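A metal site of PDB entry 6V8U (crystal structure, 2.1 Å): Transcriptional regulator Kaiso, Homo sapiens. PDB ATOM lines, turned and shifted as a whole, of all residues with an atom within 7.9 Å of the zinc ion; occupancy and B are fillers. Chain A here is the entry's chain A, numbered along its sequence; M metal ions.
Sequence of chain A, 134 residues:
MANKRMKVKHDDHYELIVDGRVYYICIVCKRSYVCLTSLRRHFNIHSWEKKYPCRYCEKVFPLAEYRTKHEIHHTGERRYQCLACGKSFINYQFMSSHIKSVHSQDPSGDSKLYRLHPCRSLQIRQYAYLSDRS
NE2 of His 98 is bound to the zinc ion (2.1 Å).
A ring nitrogen (NE2) of His 103 binds the zinc ion, at 2.1 Å.
SG of Cys 82 binds the zinc ion (2.3 Å).
SG of Cys 85 binds the zinc ion, 2.3 Å away.
The zinc ion has four donor atoms within binding distance.
Of the 15 residues printed, 4 come within 4 Å of the zinc ion.
Along chain A the residues within 4 Å of the zinc ion span positions 82 to 103.
The side-chain sulfur of Cys 82 sits close to the backbone NH of Ala 84, at 3.3 Å.
The backbone NH (N) of Lys 87 sits close to the side-chain sulfur (SG) of Cys 85.
N of Cys 82 sits at hydrogen-bond distance from O of Lys 87.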
ATOM      1  N   GLN A  81      -8.815  -4.886  -5.083  1.00  0.00           N
ATOM      2  CA  GLN A  81      -9.198  -3.565  -5.586  1.00  0.00           C
ATOM      3  C   GLN A  81      -9.144  -2.509  -4.482  1.00  0.00           C
ATOM      4  O   GLN A  81      -9.786  -2.654  -3.441  1.00  0.00           O
ATOM      5  CB  GLN A  81     -10.601  -3.588  -6.210  1.00  0.00           C
ATOM      6  CG  GLN A  81     -11.030  -2.206  -6.779  1.00  0.00           C
ATOM      7  CD  GLN A  81     -12.205  -2.300  -7.736  1.00  0.00           C
ATOM      8  OE1 GLN A  81     -13.110  -3.115  -7.527  1.00  0.00           O
ATOM      9  NE2 GLN A  81     -12.225  -1.446  -8.759  1.00  0.00           N
ATOM     10  N   CYS A  82      -8.392  -1.434  -4.727  1.00  0.00           N
ATOM     11  CA  CYS A  82      -8.421  -0.273  -3.851  1.00  0.00           C
ATOM     12  C   CYS A  82      -9.776   0.412  -3.947  1.00  0.00           C
ATOM     13  O   CYS A  82     -10.235   0.734  -5.058  1.00  0.00           O
ATOM     14  CB  CYS A  82      -7.294   0.691  -4.233  1.00  0.00           C
ATOM     15  SG  CYS A  82      -7.407   2.364  -3.484  1.00  0.00           S
ATOM     16  N   LEU A  83     -10.434   0.623  -2.812  1.00  0.00           N
ATOM     17  CA  LEU A  83     -11.748   1.255  -2.850  1.00  0.00           C
ATOM     18  C   LEU A  83     -11.676   2.780  -2.874  1.00  0.00           C
ATOM     19  O   LEU A  83     -12.718   3.435  -3.051  1.00  0.00           O
ATOM     20  CB  LEU A  83     -12.606   0.812  -1.671  1.00  0.00           C
ATOM     21  CG  LEU A  83     -12.993  -0.663  -1.685  1.00  0.00           C
ATOM     22  CD1 LEU A  83     -13.979  -0.957  -0.570  1.00  0.00           C
ATOM     23  CD2 LEU A  83     -13.584  -1.064  -3.047  1.00  0.00           C
ATOM     24  N   ALA A  84     -10.488   3.359  -2.719  1.00  0.00           N
ATOM     25  CA  ALA A  84     -10.376   4.809  -2.749  1.00  0.00           C
ATOM     26  C   ALA A  84     -10.291   5.347  -4.168  1.00  0.00           C
ATOM     27  O   ALA A  84     -10.798   6.434  -4.447  1.00  0.00           O
ATOM     28  CB  ALA A  84      -9.158   5.239  -1.926  1.00  0.00           C
ATOM     29  N   CYS A  85      -9.671   4.602  -5.094  1.00  0.00           N
ATOM     30  CA  CYS A  85      -9.537   5.058  -6.469  1.00  0.00           C
ATOM     31  C   CYS A  85      -9.881   3.997  -7.496  1.00  0.00           C
ATOM     32  O   CYS A  85      -9.930   4.327  -8.689  1.00  0.00           O
ATOM     33  CB  CYS A  85      -8.098   5.518  -6.740  1.00  0.00           C
ATOM     34  SG  CYS A  85      -6.952   4.132  -6.896  1.00  0.00           S
ATOM     35  N   GLY A  86     -10.095   2.752  -7.098  1.00  0.00           N
ATOM     36  CA  GLY A  86     -10.553   1.732  -8.006  1.00  0.00           C
ATOM     37  C   GLY A  86      -9.471   0.904  -8.691  1.00  0.00           C
ATOM     38  O   GLY A  86      -9.820  -0.025  -9.424  1.00  0.00           O
ATOM     39  N   LYS A  87      -8.192   1.205  -8.474  1.00  0.00           N
ATOM     40  CA  LYS A  87      -7.120   0.432  -9.086  1.00  0.00           C
ATOM     41  C   LYS A  87      -7.080  -0.970  -8.491  1.00  0.00           C
ATOM     42  O   LYS A  87      -7.375  -1.164  -7.312  1.00  0.00           O
ATOM     43  CB  LYS A  87      -5.768   1.107  -8.898  1.00  0.00           C
ATOM     44  CG  LYS A  87      -5.616   2.360  -9.751  1.00  0.00           C
ATOM     45  CD  LYS A  87      -4.217   2.945  -9.709  1.00  0.00           C
ATOM     46  CE  LYS A  87      -4.211   4.309 -10.418  1.00  0.00           C
ATOM     47  NZ  LYS A  87      -2.841   4.722 -10.790  1.00  0.00           N
ATOM     48  N   SER A  88      -6.702  -1.946  -9.306  1.00  0.00           N
ATOM     49  CA  SER A  88      -6.670  -3.339  -8.865  1.00  0.00           C
ATOM     50  C   SER A  88      -5.250  -3.893  -8.924  1.00  0.00           C
ATOM     51  O   SER A  88      -4.408  -3.425  -9.701  1.00  0.00           O
ATOM     52  CB  SER A  88      -7.607  -4.179  -9.729  1.00  0.00           C
ATOM     53  OG  SER A  88      -8.893  -3.591  -9.735  1.00  0.00           O
ATOM     54  N   PHE A  89      -5.002  -4.922  -8.116  1.00  0.00           N
ATOM     55  CA  PHE A  89      -3.648  -5.402  -7.829  1.00  0.00           C
ATOM     56  C   PHE A  89      -3.674  -6.927  -7.701  1.00  0.00           C
ATOM     57  O   PHE A  89      -4.679  -7.515  -7.302  1.00  0.00           O
ATOM     58  CB  PHE A  89      -3.097  -4.749  -6.513  1.00  0.00           C
ATOM     59  CG  PHE A  89      -3.035  -3.256  -6.606  1.00  0.00           C
ATOM     60  CD1 PHE A  89      -1.956  -2.637  -7.227  1.00  0.00           C
ATOM     61  CD2 PHE A  89      -4.084  -2.467  -6.149  1.00  0.00           C
ATOM     62  CE1 PHE A  89      -1.908  -1.255  -7.366  1.00  0.00           C
ATOM     63  CE2 PHE A  89      -4.041  -1.079  -6.294  1.00  0.00           C
ATOM     64  CZ  PHE A  89      -2.956  -0.474  -6.916  1.00  0.00           C
ATOM     65  N   MET A  95      -1.441  -4.038  -3.211  1.00  0.00           N
ATOM     66  CA  MET A  95      -2.588  -3.250  -2.777  1.00  0.00           C
ATOM     67  C   MET A  95      -2.228  -2.442  -1.536  1.00  0.00           C
ATOM     68  O   MET A  95      -2.491  -1.231  -1.460  1.00  0.00           O
ATOM     69  CB  MET A  95      -3.766  -4.193  -2.492  1.00  0.00           C
ATOM     70  CG  MET A  95      -4.988  -3.583  -1.787  1.00  0.00           C
ATOM     71  SD  MET A  95      -4.804  -3.302   0.013  1.00  0.00           S
ATOM     72  CE  MET A  95      -4.520  -4.945   0.704  1.00  0.00           C
ATOM     73  N   HIS A  98       0.188   0.352  -2.291  1.00  0.00           N
ATOM     74  CA  HIS A  98      -0.483   1.436  -3.009  1.00  0.00           C
ATOM     75  C   HIS A  98      -1.278   2.308  -2.042  1.00  0.00           C
ATOM     76  O   HIS A  98      -1.223   3.544  -2.105  1.00  0.00           O
ATOM     77  CB  HIS A  98      -1.406   0.876  -4.099  1.00  0.00           C
ATOM     78  CG  HIS A  98      -2.425   1.864  -4.583  1.00  0.00           C
ATOM     79  ND1 HIS A  98      -2.160   2.809  -5.555  1.00  0.00           N
ATOM     80  CD2 HIS A  98      -3.723   2.067  -4.214  1.00  0.00           C
ATOM     81  CE1 HIS A  98      -3.246   3.546  -5.764  1.00  0.00           C
ATOM     82  NE2 HIS A  98      -4.199   3.117  -4.965  1.00  0.00           N
ATOM     83  N   ILE A  99      -2.056   1.679  -1.168  1.00  0.00           N
ATOM     84  CA  ILE A  99      -2.935   2.443  -0.286  1.00  0.00           C
ATOM     85  C   ILE A  99      -2.117   3.246   0.720  1.00  0.00           C
ATOM     86  O   ILE A  99      -2.448   4.398   1.034  1.00  0.00           O
ATOM     87  CB  ILE A  99      -3.955   1.496   0.374  1.00  0.00           C
ATOM     88  CG1 ILE A  99      -4.863   0.889  -0.695  1.00  0.00           C
ATOM     89  CG2 ILE A  99      -4.768   2.243   1.438  1.00  0.00           C
ATOM     90  CD1 ILE A  99      -6.019   0.021  -0.142  1.00  0.00           C
ATOM     91  N   VAL A 102      -0.066   6.078  -1.705  1.00  0.00           N
ATOM     92  CA  VAL A 102      -0.888   7.012  -2.486  1.00  0.00           C
ATOM     93  C   VAL A 102      -1.994   7.618  -1.636  1.00  0.00           C
ATOM     94  O   VAL A 102      -2.327   8.786  -1.795  1.00  0.00           O
ATOM     95  CB  VAL A 102      -1.474   6.312  -3.729  1.00  0.00           C
ATOM     96  CG1 VAL A 102      -2.459   7.271  -4.494  1.00  0.00           C
ATOM     97  CG2 VAL A 102      -0.356   5.850  -4.638  1.00  0.00           C
ATOM     98  N   HIS A 103      -2.568   6.856  -0.722  1.00  0.00           N
ATOM     99  CA  HIS A 103      -3.704   7.331   0.043  1.00  0.00           C
ATOM    100  C   HIS A 103      -3.387   7.602   1.510  1.00  0.00           C
ATOM    101  O   HIS A 103      -4.250   8.136   2.214  1.00  0.00           O
ATOM    102  CB  HIS A 103      -4.863   6.336  -0.101  1.00  0.00           C
ATOM    103  CG  HIS A 103      -5.329   6.186  -1.520  1.00  0.00           C
ATOM    104  ND1 HIS A 103      -5.765   7.259  -2.261  1.00  0.00           N
ATOM    105  CD2 HIS A 103      -5.406   5.110  -2.335  1.00  0.00           C
ATOM    106  CE1 HIS A 103      -6.096   6.843  -3.468  1.00  0.00           C
ATOM    107  NE2 HIS A 103      -5.886   5.542  -3.544  1.00  0.00           N
ATOM    108  N   LEU A 113     -10.647  -0.686   3.366  1.00  0.00           N
ATOM    109  CA  LEU A 113     -10.161   0.153   2.279  1.00  0.00           C
ATOM    110  C   LEU A 113      -9.961  -0.610   0.974  1.00  0.00           C
ATOM    111  O   LEU A 113      -9.631   0.011  -0.036  1.00  0.00           O
ATOM    112  CB  LEU A 113      -8.833   0.803   2.675  1.00  0.00           C
ATOM    113  CG  LEU A 113      -8.918   1.503   4.040  1.00  0.00           C
ATOM    114  CD1 LEU A 113      -7.598   2.119   4.442  1.00  0.00           C
ATOM    115  CD2 LEU A 113      -9.989   2.576   3.993  1.00  0.00           C
HETATM  116 ZN    ZN M   1      -6.130   3.787  -4.730  1.00  0.00          ZN
